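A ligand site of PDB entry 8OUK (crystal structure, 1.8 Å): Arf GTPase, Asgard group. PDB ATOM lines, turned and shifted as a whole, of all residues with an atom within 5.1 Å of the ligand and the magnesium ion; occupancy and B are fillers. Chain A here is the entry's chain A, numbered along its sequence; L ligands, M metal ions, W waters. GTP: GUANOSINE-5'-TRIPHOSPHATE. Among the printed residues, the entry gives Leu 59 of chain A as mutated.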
ATOM      1  N   GLY A  11      -1.053 -13.520   7.776  1.00  0.00           N
ATOM      2  CA  GLY A  11      -0.535 -12.209   7.426  1.00  0.00           C
ATOM      3  C   GLY A  11       0.752 -12.388   6.672  1.00  0.00           C
ATOM      4  O   GLY A  11       1.351 -13.480   6.685  1.00  0.00           O
ATOM      5  N   LEU A  12       1.208 -11.336   5.983  1.00  0.00           N
ATOM      6  CA  LEU A  12       2.408 -11.452   5.173  1.00  0.00           C
ATOM      7  C   LEU A  12       3.616 -11.784   6.027  1.00  0.00           C
ATOM      8  O   LEU A  12       3.635 -11.511   7.239  1.00  0.00           O
ATOM      9  CB  LEU A  12       2.671 -10.144   4.402  1.00  0.00           C
ATOM     10  CG  LEU A  12       1.561  -9.607   3.501  1.00  0.00           C
ATOM     11  CD1 LEU A  12       2.112  -8.417   2.711  1.00  0.00           C
ATOM     12  CD2 LEU A  12       1.041 -10.681   2.516  1.00  0.00           C
ATOM     13  N   ASP A  13       4.668 -12.295   5.390  1.00  0.00           N
ATOM     14  CA  ASP A  13       5.951 -12.534   6.046  1.00  0.00           C
ATOM     15  C   ASP A  13       6.459 -11.158   6.574  1.00  0.00           C
ATOM     16  O   ASP A  13       6.173 -10.121   5.935  1.00  0.00           O
ATOM     17  CB  ASP A  13       6.961 -13.094   5.022  1.00  0.00           C
ATOM     18  CG  ASP A  13       7.051 -12.268   3.738  1.00  0.00           C
ATOM     19  OD1 ASP A  13       6.128 -12.394   2.894  1.00  0.00           O
ATOM     20  OD2 ASP A  13       8.020 -11.484   3.605  1.00  0.00           O
ATOM     21  N   TYR A  14       7.033 -11.143   7.769  1.00  0.00           N
ATOM     22  CA  TYR A  14       7.570  -9.960   8.434  1.00  0.00           C
ATOM     23  C   TYR A  14       6.491  -9.090   9.121  1.00  0.00           C
ATOM     24  O   TYR A  14       6.850  -8.062   9.698  1.00  0.00           O
ATOM     25  CB  TYR A  14       8.416  -9.116   7.452  1.00  0.00           C
ATOM     26  CG  TYR A  14       9.631  -8.486   8.085  1.00  0.00           C
ATOM     27  CD1 TYR A  14      10.742  -9.248   8.423  1.00  0.00           C
ATOM     28  CD2 TYR A  14       9.680  -7.115   8.331  1.00  0.00           C
ATOM     29  CE1 TYR A  14      11.874  -8.656   8.978  1.00  0.00           C
ATOM     30  CE2 TYR A  14      10.798  -6.522   8.897  1.00  0.00           C
ATOM     31  CZ  TYR A  14      11.888  -7.306   9.236  1.00  0.00           C
ATOM     32  OH  TYR A  14      13.013  -6.721   9.792  1.00  0.00           O
ATOM     33  N   ALA A  15       5.218  -9.492   9.111  1.00  0.00           N
ATOM     34  CA  ALA A  15       4.155  -8.683   9.743  1.00  0.00           C
ATOM     35  C   ALA A  15       4.295  -8.607  11.262  1.00  0.00           C
ATOM     36  O   ALA A  15       3.925  -7.598  11.859  1.00  0.00           O
ATOM     37  CB  ALA A  15       2.774  -9.233   9.374  1.00  0.00           C
ATOM     38  N   GLY A  16       4.829  -9.672  11.874  1.00  0.00           N
ATOM     39  CA  GLY A  16       5.058  -9.729  13.305  1.00  0.00           C
ATOM     40  C   GLY A  16       4.277 -10.789  14.044  1.00  0.00           C
ATOM     41  O   GLY A  16       4.184 -10.753  15.275  1.00  0.00           O
ATOM     42  N   LYS A  17       3.690 -11.767  13.311  1.00  0.00           N
ATOM     43  CA  LYS A  17       2.894 -12.821  13.959  1.00  0.00           C
ATOM     44  C   LYS A  17       3.671 -13.565  15.077  1.00  0.00           C
ATOM     45  O   LYS A  17       3.181 -13.673  16.199  1.00  0.00           O
ATOM     46  CB  LYS A  17       2.408 -13.864  12.911  1.00  0.00           C
ATOM     47  CG  LYS A  17       1.649 -13.252  11.734  1.00  0.00           C
ATOM     48  CD  LYS A  17       1.285 -14.341  10.670  1.00  0.00           C
ATOM     49  CE  LYS A  17       2.508 -14.897   9.948  1.00  0.00           C
ATOM     50  NZ  LYS A  17       3.178 -13.882   9.051  1.00  0.00           N
ATOM     51  N   SER A  18       4.850 -14.075  14.742  1.00  0.00           N
ATOM     52  CA  SER A  18       5.636 -14.838  15.711  1.00  0.00           C
ATOM     53  C   SER A  18       6.071 -13.957  16.883  1.00  0.00           C
ATOM     54  O   SER A  18       6.067 -14.409  18.014  1.00  0.00           O
ATOM     55  CB  SER A  18       6.847 -15.461  15.034  1.00  0.00           C
ATOM     56  OG  SER A  18       6.444 -16.259  13.915  1.00  0.00           O
ATOM     57  N   THR A  19       6.443 -12.710  16.609  1.00  0.00           N
ATOM     58  CA  THR A  19       6.869 -11.789  17.667  1.00  0.00           C
ATOM     59  C   THR A  19       5.725 -11.450  18.659  1.00  0.00           C
ATOM     60  O   THR A  19       5.950 -11.396  19.879  1.00  0.00           O
ATOM     61  CB  THR A  19       7.474 -10.543  17.022  1.00  0.00           C
ATOM     62  OG1 THR A  19       8.515 -10.940  16.145  1.00  0.00           O
ATOM     63  CG2 THR A  19       8.026  -9.563  18.055  1.00  0.00           C
ATOM     64  N   PHE A  29       9.923  -8.920  24.298  1.00  0.00           N
ATOM     65  CA  PHE A  29       9.978  -8.510  22.899  1.00  0.00           C
ATOM     66  C   PHE A  29      11.275  -8.963  22.258  1.00  0.00           C
ATOM     67  O   PHE A  29      12.359  -8.606  22.743  1.00  0.00           O
ATOM     68  CB  PHE A  29       9.830  -6.987  22.751  1.00  0.00           C
ATOM     69  CG  PHE A  29      10.149  -6.422  21.390  1.00  0.00           C
ATOM     70  CD1 PHE A  29       9.427  -6.826  20.268  1.00  0.00           C
ATOM     71  CD2 PHE A  29      11.118  -5.448  21.231  1.00  0.00           C
ATOM     72  CE1 PHE A  29       9.711  -6.289  19.010  1.00  0.00           C
ATOM     73  CE2 PHE A  29      11.387  -4.912  19.973  1.00  0.00           C
ATOM     74  CZ  PHE A  29      10.696  -5.356  18.874  1.00  0.00           C
ATOM     75  N   SER A  30      11.183  -9.732  21.169  1.00  0.00           N
ATOM     76  CA  SER A  30      12.391 -10.098  20.430  1.00  0.00           C
ATOM     77  C   SER A  30      12.410  -9.258  19.175  1.00  0.00           C
ATOM     78  O   SER A  30      11.515  -9.368  18.339  1.00  0.00           O
ATOM     79  CB  SER A  30      12.467 -11.591  20.123  1.00  0.00           C
ATOM     80  OG  SER A  30      11.203 -12.240  20.044  1.00  0.00           O
ATOM     81  N   ASP A  31      13.382  -8.366  19.063  1.00  0.00           N
ATOM     82  CA  ASP A  31      13.520  -7.508  17.888  1.00  0.00           C
ATOM     83  C   ASP A  31      14.231  -8.212  16.714  1.00  0.00           C
ATOM     84  O   ASP A  31      14.344  -7.624  15.632  1.00  0.00           O
ATOM     85  CB  ASP A  31      14.272  -6.220  18.264  1.00  0.00           C
ATOM     86  CG  ASP A  31      15.695  -6.424  18.766  1.00  0.00           C
ATOM     87  OD1 ASP A  31      16.106  -7.603  18.926  1.00  0.00           O
ATOM     88  OD2 ASP A  31      16.380  -5.411  19.024  1.00  0.00           O
ATOM     89  N   ASP A  32      14.674  -9.471  16.911  1.00  0.00           N
ATOM     90  CA  ASP A  32      15.423 -10.235  15.943  1.00  0.00           C
ATOM     91  C   ASP A  32      14.786 -11.585  15.623  1.00  0.00           C
ATOM     92  O   ASP A  32      15.514 -12.536  15.303  1.00  0.00           O
ATOM     93  CB  ASP A  32      16.860 -10.450  16.477  1.00  0.00           C
ATOM     94  CG  ASP A  32      16.950 -11.151  17.820  1.00  0.00           C
ATOM     95  OD1 ASP A  32      15.886 -11.436  18.434  1.00  0.00           O
ATOM     96  OD2 ASP A  32      18.100 -11.432  18.279  1.00  0.00           O
ATOM     97  N   THR A  33      13.445 -11.670  15.697  1.00  0.00           N
ATOM     98  CA  THR A  33      12.704 -12.893  15.416  1.00  0.00           C
ATOM     99  C   THR A  33      13.012 -13.389  14.014  1.00  0.00           C
ATOM    100  O   THR A  33      13.053 -12.600  13.075  1.00  0.00           O
ATOM    101  CB  THR A  33      11.202 -12.658  15.563  1.00  0.00           C
ATOM    102  OG1 THR A  33      10.939 -12.010  16.813  1.00  0.00           O
ATOM    103  CG2 THR A  33      10.387 -13.962  15.449  1.00  0.00           C
ATOM    104  N   LYS A  34      13.258 -14.698  13.883  1.00  0.00           N
ATOM    105  CA  LYS A  34      13.617 -15.261  12.596  1.00  0.00           C
ATOM    106  C   LYS A  34      12.411 -15.745  11.841  1.00  0.00           C
ATOM    107  O   LYS A  34      11.429 -16.163  12.455  1.00  0.00           O
ATOM    108  CB  LYS A  34      14.636 -16.401  12.785  1.00  0.00           C
ATOM    109  CG  LYS A  34      15.859 -15.979  13.636  1.00  0.00           C
ATOM    110  CD  LYS A  34      16.637 -14.825  13.009  1.00  0.00           C
ATOM    111  CE  LYS A  34      17.900 -14.513  13.799  1.00  0.00           C
ATOM    112  NZ  LYS A  34      17.616 -14.472  15.260  1.00  0.00           N
ATOM    113  N   ARG A  35      12.493 -15.684  10.501  1.00  0.00           N
ATOM    114  CA  ARG A  35      11.419 -16.112   9.591  1.00  0.00           C
ATOM    115  C   ARG A  35      10.940 -17.531   9.899  1.00  0.00           C
ATOM    116  O   ARG A  35      11.759 -18.444  10.088  1.00  0.00           O
ATOM    117  CB  ARG A  35      11.887 -15.982   8.136  1.00  0.00           C
ATOM    118  CG  ARG A  35      10.895 -16.523   7.115  1.00  0.00           C
ATOM    119  CD  ARG A  35      11.375 -16.333   5.706  1.00  0.00           C
ATOM    120  NE  ARG A  35      11.451 -14.928   5.317  1.00  0.00           N
ATOM    121  CZ  ARG A  35      12.050 -14.480   4.218  1.00  0.00           C
ATOM    122  NH1 ARG A  35      12.682 -15.327   3.407  1.00  0.00           N
ATOM    123  NH2 ARG A  35      12.059 -13.183   3.929  1.00  0.00           N
ATOM    124  N   THR A  36       9.617 -17.719   9.932  1.00  0.00           N
ATOM    125  CA  THR A  36       9.006 -19.002  10.218  1.00  0.00           C
ATOM    126  C   THR A  36       8.985 -19.814   8.931  1.00  0.00           C
ATOM    127  O   THR A  36       8.445 -19.364   7.929  1.00  0.00           O
ATOM    128  CB  THR A  36       7.611 -18.791  10.809  1.00  0.00           C
ATOM    129  OG1 THR A  36       7.747 -18.025  12.010  1.00  0.00           O
ATOM    130  CG2 THR A  36       6.868 -20.114  11.108  1.00  0.00           C
ATOM    131  N   ASN A  40       4.514 -22.852  13.609  1.00  0.00           N
ATOM    132  CA  ASN A  40       4.839 -22.835  15.024  1.00  0.00           C
ATOM    133  C   ASN A  40       3.519 -23.093  15.744  1.00  0.00           C
ATOM    134  O   ASN A  40       2.504 -22.447  15.427  1.00  0.00           O
ATOM    135  CB  ASN A  40       5.363 -21.480  15.464  1.00  0.00           C
ATOM    136  CG  ASN A  40       6.747 -21.208  14.973  1.00  0.00           C
ATOM    137  OD1 ASN A  40       7.587 -22.123  14.871  1.00  0.00           O
ATOM    138  ND2 ASN A  40       7.019 -19.952  14.668  1.00  0.00           N
ATOM    139  N   ASP A  55       0.727 -20.509  14.166  1.00  0.00           N
ATOM    140  CA  ASP A  55       1.472 -19.402  13.583  1.00  0.00           C
ATOM    141  C   ASP A  55       2.093 -19.947  12.316  1.00  0.00           C
ATOM    142  O   ASP A  55       3.062 -20.724  12.364  1.00  0.00           O
ATOM    143  CB  ASP A  55       2.510 -18.944  14.601  1.00  0.00           C
ATOM    144  CG  ASP A  55       3.579 -18.000  14.054  1.00  0.00           C
ATOM    145  OD1 ASP A  55       3.322 -17.364  13.026  1.00  0.00           O
ATOM    146  OD2 ASP A  55       4.667 -17.938  14.653  1.00  0.00           O
ATOM    147  N   ILE A  56       1.520 -19.573  11.179  1.00  0.00           N
ATOM    148  CA  ILE A  56       1.950 -20.133   9.903  1.00  0.00           C
ATOM    149  C   ILE A  56       2.834 -19.149   9.221  1.00  0.00           C
ATOM    150  O   ILE A  56       2.507 -17.959   9.160  1.00  0.00           O
ATOM    151  CB  ILE A  56       0.711 -20.513   9.038  1.00  0.00           C
ATOM    152  CG1 ILE A  56      -0.372 -21.259   9.850  1.00  0.00           C
ATOM    153  CG2 ILE A  56       1.109 -21.353   7.825  1.00  0.00           C
ATOM    154  CD1 ILE A  56      -1.708 -20.521   9.835  1.00  0.00           C
ATOM    155  N   GLY A  57       3.940 -19.628   8.621  1.00  0.00           N
ATOM    156  CA  GLY A  57       4.821 -18.758   7.848  1.00  0.00           C
ATOM    157  C   GLY A  57       4.070 -17.981   6.778  1.00  0.00           C
ATOM    158  O   GLY A  57       3.177 -18.531   6.109  1.00  0.00           O
ATOM    159  N   GLY A  58       4.370 -16.710   6.642  1.00  0.00           N
ATOM    160  CA  GLY A  58       3.687 -15.849   5.695  1.00  0.00           C
ATOM    161  C   GLY A  58       4.355 -15.745   4.354  1.00  0.00           C
ATOM    162  O   GLY A  58       3.820 -15.057   3.482  1.00  0.00           O
ATOM    163  N   LEU A  59       5.518 -16.395   4.140  1.00  0.00           N
ATOM    164  CA  LEU A  59       6.181 -16.352   2.834  1.00  0.00           C
ATOM    165  C   LEU A  59       5.264 -17.020   1.793  1.00  0.00           C
ATOM    166  O   LEU A  59       4.454 -17.879   2.154  1.00  0.00           O
ATOM    167  CB  LEU A  59       7.531 -17.088   2.869  1.00  0.00           C
ATOM    168  CG  LEU A  59       8.594 -16.553   1.924  1.00  0.00           C
ATOM    169  CD1 LEU A  59       8.965 -15.089   2.284  1.00  0.00           C
ATOM    170  CD2 LEU A  59       9.831 -17.473   1.924  1.00  0.00           C
ATOM    171  N   ASN A 116      -0.106  -3.955  13.460  1.00  0.00           N
ATOM    172  CA  ASN A 116       1.068  -4.118  14.300  1.00  0.00           C
ATOM    173  C   ASN A 116       2.198  -3.096  14.056  1.00  0.00           C
ATOM    174  O   ASN A 116       2.148  -2.334  13.089  1.00  0.00           O
ATOM    175  CB  ASN A 116       1.581  -5.567  14.161  1.00  0.00           C
ATOM    176  CG  ASN A 116       2.607  -5.960  15.200  1.00  0.00           C
ATOM    177  OD1 ASN A 116       2.494  -5.569  16.362  1.00  0.00           O
ATOM    178  ND2 ASN A 116       3.618  -6.717  14.795  1.00  0.00           N
ATOM    179  N   LYS A 117       3.188  -3.068  14.980  1.00  0.00           N
ATOM    180  CA  LYS A 117       4.380  -2.199  14.910  1.00  0.00           C
ATOM    181  C   LYS A 117       4.043  -0.720  15.077  1.00  0.00           C
ATOM    182  O   LYS A 117       4.726   0.131  14.515  1.00  0.00           O
ATOM    183  CB  LYS A 117       5.217  -2.467  13.630  1.00  0.00           C
ATOM    184  CG  LYS A 117       5.435  -3.968  13.335  1.00  0.00           C
ATOM    185  CD  LYS A 117       6.731  -4.215  12.526  1.00  0.00           C
ATOM    186  CE  LYS A 117       6.797  -5.636  11.983  1.00  0.00           C
ATOM    187  NZ  LYS A 117       7.842  -5.766  10.903  1.00  0.00           N
ATOM    188  N   GLN A 118       2.998  -0.407  15.881  1.00  0.00           N
ATOM    189  CA  GLN A 118       2.622   0.993  16.154  1.00  0.00           C
ATOM    190  C   GLN A 118       3.710   1.815  16.840  1.00  0.00           C
ATOM    191  O   GLN A 118       3.643   3.056  16.847  1.00  0.00           O
ATOM    192  CB  GLN A 118       1.339   1.052  16.988  1.00  0.00           C
ATOM    193  CG  GLN A 118       0.090   0.581  16.242  1.00  0.00           C
ATOM    194  CD  GLN A 118      -0.256   1.495  15.101  1.00  0.00           C
ATOM    195  OE1 GLN A 118      -0.166   2.723  15.219  1.00  0.00           O
ATOM    196  NE2 GLN A 118      -0.625   0.925  13.963  1.00  0.00           N
ATOM    197  N   ASP A 119       4.697   1.134  17.432  1.00  0.00           N
ATOM    198  CA  ASP A 119       5.819   1.813  18.090  1.00  0.00           C
ATOM    199  C   ASP A 119       6.764   2.464  17.065  1.00  0.00           C
ATOM    200  O   ASP A 119       7.517   3.368  17.433  1.00  0.00           O
ATOM    201  CB  ASP A 119       6.600   0.796  18.920  1.00  0.00           C
ATOM    202  CG  ASP A 119       7.137  -0.349  18.074  1.00  0.00           C
ATOM    203  OD1 ASP A 119       6.320  -1.235  17.685  1.00  0.00           O
ATOM    204  OD2 ASP A 119       8.340  -0.356  17.797  1.00  0.00           O
ATOM    205  N   LEU A 120       6.766   2.003  15.799  1.00  0.00           N
ATOM    206  CA  LEU A 120       7.687   2.542  14.793  1.00  0.00           C
ATOM    207  C   LEU A 120       7.234   3.894  14.267  1.00  0.00           C
ATOM    208  O   LEU A 120       6.030   4.115  14.125  1.00  0.00           O
ATOM    209  CB  LEU A 120       7.894   1.531  13.654  1.00  0.00           C
ATOM    210  CG  LEU A 120       8.565   0.212  14.057  1.00  0.00           C
ATOM    211  CD1 LEU A 120       8.606  -0.743  12.893  1.00  0.00           C
ATOM    212  CD2 LEU A 120       9.986   0.451  14.593  1.00  0.00           C
ATOM    213  N   CYS A 148      -1.666  -2.273  17.439  1.00  0.00           N
ATOM    214  CA  CYS A 148      -0.900  -2.886  18.516  1.00  0.00           C
ATOM    215  C   CYS A 148       0.617  -2.784  18.301  1.00  0.00           C
ATOM    216  O   CYS A 148       1.081  -2.315  17.259  1.00  0.00           O
ATOM    217  CB  CYS A 148      -1.342  -4.335  18.697  1.00  0.00           C
ATOM    218  SG  CYS A 148      -0.908  -5.402  17.302  1.00  0.00           S
ATOM    219  N   SER A 149       1.390  -3.204  19.312  1.00  0.00           N
ATOM    220  CA  SER A 149       2.843  -3.265  19.210  1.00  0.00           C
ATOM    221  C   SER A 149       3.346  -4.434  20.042  1.00  0.00           C
ATOM    222  O   SER A 149       3.059  -4.494  21.230  1.00  0.00           O
ATOM    223  CB  SER A 149       3.475  -1.978  19.726  1.00  0.00           C
ATOM    224  OG  SER A 149       4.896  -2.135  19.763  1.00  0.00           O
ATOM    225  N   ALA A 150       4.122  -5.344  19.438  1.00  0.00           N
ATOM    226  CA  ALA A 150       4.770  -6.405  20.211  1.00  0.00           C
ATOM    227  C   ALA A 150       5.937  -5.797  21.026  1.00  0.00           C
ATOM    228  O   ALA A 150       6.369  -6.395  22.010  1.00  0.00           O
ATOM    229  CB  ALA A 150       5.325  -7.479  19.279  1.00  0.00           C
ATOM    230  N   ALA A 151       6.496  -4.657  20.571  1.00  0.00           N
ATOM    231  CA  ALA A 151       7.604  -3.993  21.231  1.00  0.00           C
ATOM    232  C   ALA A 151       7.222  -3.405  22.575  1.00  0.00           C
ATOM    233  O   ALA A 151       7.957  -3.558  23.563  1.00  0.00           O
ATOM    234  CB  ALA A 151       8.202  -2.940  20.321  1.00  0.00           C
HETATM  235  PG  GTP L   1       6.972 -14.893   8.966  1.00  0.00           P
HETATM  236  O1G GTP L   1       5.563 -15.246   8.680  1.00  0.00           O
HETATM  237  O2G GTP L   1       7.836 -14.714   7.759  1.00  0.00           O
HETATM  238  O3G GTP L   1       7.585 -15.751   9.982  1.00  0.00           O
HETATM  239  O3B GTP L   1       6.948 -13.457   9.678  1.00  0.00           O
HETATM  240  PB  GTP L   1       6.217 -12.982  11.011  1.00  0.00           P
HETATM  241  O1B GTP L   1       4.874 -12.438  10.711  1.00  0.00           O
HETATM  242  O2B GTP L   1       6.159 -14.105  12.028  1.00  0.00           O
HETATM  243  O3A GTP L   1       7.100 -11.773  11.575  1.00  0.00           O
HETATM  244  PA  GTP L   1       8.203 -11.750  12.720  1.00  0.00           P
HETATM  245  O1A GTP L   1       9.286 -12.717  12.402  1.00  0.00           O
HETATM  246  O2A GTP L   1       7.494 -12.063  14.038  1.00  0.00           O
HETATM  247  O5' GTP L   1       8.650 -10.230  12.784  1.00  0.00           O
HETATM  248  C5' GTP L   1       9.378  -9.641  11.693  1.00  0.00           C
HETATM  249  C4' GTP L   1      10.295  -8.587  12.270  1.00  0.00           C
HETATM  250  O4' GTP L   1       9.513  -7.511  12.830  1.00  0.00           O
HETATM  251  C3' GTP L   1      11.246  -9.056  13.375  1.00  0.00           C
HETATM  252  O3' GTP L   1      12.495  -8.366  13.260  1.00  0.00           O
HETATM  253  C2' GTP L   1      10.510  -8.636  14.643  1.00  0.00           C
HETATM  254  O2' GTP L   1      11.352  -8.425  15.771  1.00  0.00           O
HETATM  255  C1' GTP L   1       9.874  -7.312  14.189  1.00  0.00           C
HETATM  256  N9  GTP L   1       8.665  -6.947  14.928  1.00  0.00           N
HETATM  257  C8  GTP L   1       7.517  -7.686  15.077  1.00  0.00           C
HETATM  258  N7  GTP L   1       6.567  -7.036  15.712  1.00  0.00           N
HETATM  259  C5  GTP L   1       7.130  -5.799  15.992  1.00  0.00           C
HETATM  260  C6  GTP L   1       6.586  -4.634  16.655  1.00  0.00           C
HETATM  261  O6  GTP L   1       5.448  -4.483  17.101  1.00  0.00           O
HETATM  262  N1  GTP L   1       7.503  -3.607  16.742  1.00  0.00           N
HETATM  263  C2  GTP L   1       8.778  -3.657  16.258  1.00  0.00           C
HETATM  264  N2  GTP L   1       9.545  -2.576  16.451  1.00  0.00           N
HETATM  265  N3  GTP L   1       9.291  -4.720  15.636  1.00  0.00           N
HETATM  266  C4  GTP L   1       8.423  -5.741  15.529  1.00  0.00           C
HETATM  267 MG    MG M   1       6.978 -15.972  11.936  1.00  0.00          MG
HETATM  268  O   HOH W   1       5.126 -16.814  11.339  1.00  0.00           O
HETATM  269  O   HOH W   2       9.959 -13.186   7.446  1.00  0.00           O
HETATM  270  O   HOH W   3      10.879 -12.589  10.007  1.00  0.00           O
HETATM  271  O   HOH W   4      10.302  -4.349  12.085  1.00  0.00           O
HETATM  272  O   HOH W   5      12.811  -5.027  12.640  1.00  0.00           O
HETATM  273  O   HOH W   6       7.556 -17.135   6.285  1.00  0.00           O
HETATM  274  O   HOH W   7       8.786 -15.301  12.627  1.00  0.00           O
HETATM  275  O   HOH W   8      12.377  -2.613  15.789  1.00  0.00           O
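Water W7 bridges an oxygen (O1A) of the ligand (2.6 Å) and the backbone carbonyl oxygen of Lys 34 (2.8 Å).
Water W1 lies within hydrogen-bond range of OD1 of Asp 55 (2.5 Å) and O1G of the ligand (3.1 Å).
Water W2 bridges O2G of the ligand (2.6 Å) and NE of Arg 35 (3.1 Å).
Water W6 lies within hydrogen-bond range of an oxygen (O2G) of the ligand (2.8 Å), the backbone carbonyl oxygen (O) of Thr 36 (2.9 Å), the backbone NH (N) of Leu 59 (3.0 Å) and the backbone NH (N) of Gly 58 (3.2 Å).
Water W4 bridges NZ of Lys 117 and O4' of the ligand.
Water W5 lies within hydrogen-bond range of OH of Tyr 14 (3.3 Å) and O3' of the ligand (3.4 Å).
The magnesium ion is bound by an oxygen (O2B) of the ligand, water W7, an oxygen (O3G) of the ligand, the side-chain hydroxyl (OG) of Ser 18, water W1 and the side-chain hydroxyl (OG1) of Thr 36.
The magnesium ion has six donor atoms within binding distance.
The nearest printed residue that does not touch the magnesium ion is Asp 55 (4.1 Å).
N of Gly 16 lies within hydrogen-bond range of O1B of the ligand, 3.0 Å away.
The side-chain amide nitrogen of Asn 116 is in hydrogen-bond range of a nitrogen (N7) of the ligand (3.1 Å).
N of Ala 15 lies within hydrogen-bond range of O1B of the ligand (3.4 Å).
The backbone carbonyl oxygen (O) of Ser 30 lies within hydrogen-bond range of an oxygen (O2') of the ligand (2.7 Å).
O of Asp 31 lies within hydrogen-bond range of O3' of the ligand, 3.1 Å away.
O3B of the ligand sits at hydrogen-bond distance from N of Tyr 14.
The backbone NH (N) of Gly 58 is in hydrogen-bond range of an oxygen (O1G) of the ligand.
O3G of the ligand lies close to N of Thr 36 (2.8 Å).
An oxygen (O2A) of the ligand lies within hydrogen-bond range of the side-chain hydroxyl of Thr 19 (2.6 Å).
NZ of Lys 17 is in salt-bridge range of O1G of the ligand, 2.8 Å away.
The backbone NH of Lys 117 sits close to an oxygen (O6) of the ligand, 3.4 Å away.
N of Ala 150 sits at hydrogen-bond distance from O6 of the ligand, 2.8 Å away.
The side-chain amino group (NZ) of Lys 117 sits at hydrogen-bond distance from an oxygen (O4') of the ligand (3.1 Å).
OD1 of Asp 119 lies within hydrogen-bond range of N1 of the ligand (2.8 Å).
O2A of the ligand is in hydrogen-bond range of N of Thr 19, at 2.9 Å.
The backbone NH (N) of Ser 18 is in hydrogen-bond range of an oxygen (O2A) of the ligand.
An oxygen (O1B) of the ligand is in hydrogen-bond range of the backbone NH (N) of Lys 17.
OG of Ser 18 lies close to OD2 of Asp 55.
The side-chain amide oxygen (OD1) of Asn 116 is in hydrogen-bond range of the side-chain sulfur (SG) of Cys 148 (3.5 Å).
OG1 of Thr 36 sits close to ND2 of Asn 40, at 3.4 Å.
O of Leu 12 is in hydrogen-bond range of NZ of Lys 17, 3.0 Å away.
The backbone carbonyl oxygen of Asp 32 is in hydrogen-bond range of the side-chain amino group of Lys 34 (2.9 Å).
The backbone carbonyl oxygen of Gly 11 is in hydrogen-bond range of the side-chain amino group of Lys 17 (3.0 Å).
The side-chain amino group (NZ) of Lys 117 is in hydrogen-bond range of the backbone carbonyl oxygen (O) of Tyr 14 (2.8 Å).
The backbone NH (N) of Ala 151 is in hydrogen-bond range of the side-chain hydroxyl (OG) of Ser 149.
Residues that only touch the ligand: Asp 13 (3.3 Å), Thr 33 (3.5 Å), Ser 149 (3.6 Å), Leu 120 (3.6 Å), Phe 29 (3.6 Å), Arg 35 (3.6 Å), Ala 151 (3.6 Å), Gly 57 (3.7 Å), Asp 32 (3.7 Å) and Leu 12 (3.8 Å).
Hydrophobic or aromatic side chains that line the ligand: Tyr 14, Phe 29, Leu 120, Ala 150 and Ala 151.
24 residues have an atom within 4 Å of the ligand: Leu 12, Asp 13, Tyr 14, Ala 15, Gly 16, Lys 17, Ser 18, Thr 19, Phe 29, Ser 30, Asp 31, Asp 32, Thr 33, Arg 35, Thr 36, Gly 57, Gly 58, Asn 116, Lys 117, Asp 119, Leu 120, Ser 149, Ala 150 and Ala 151.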
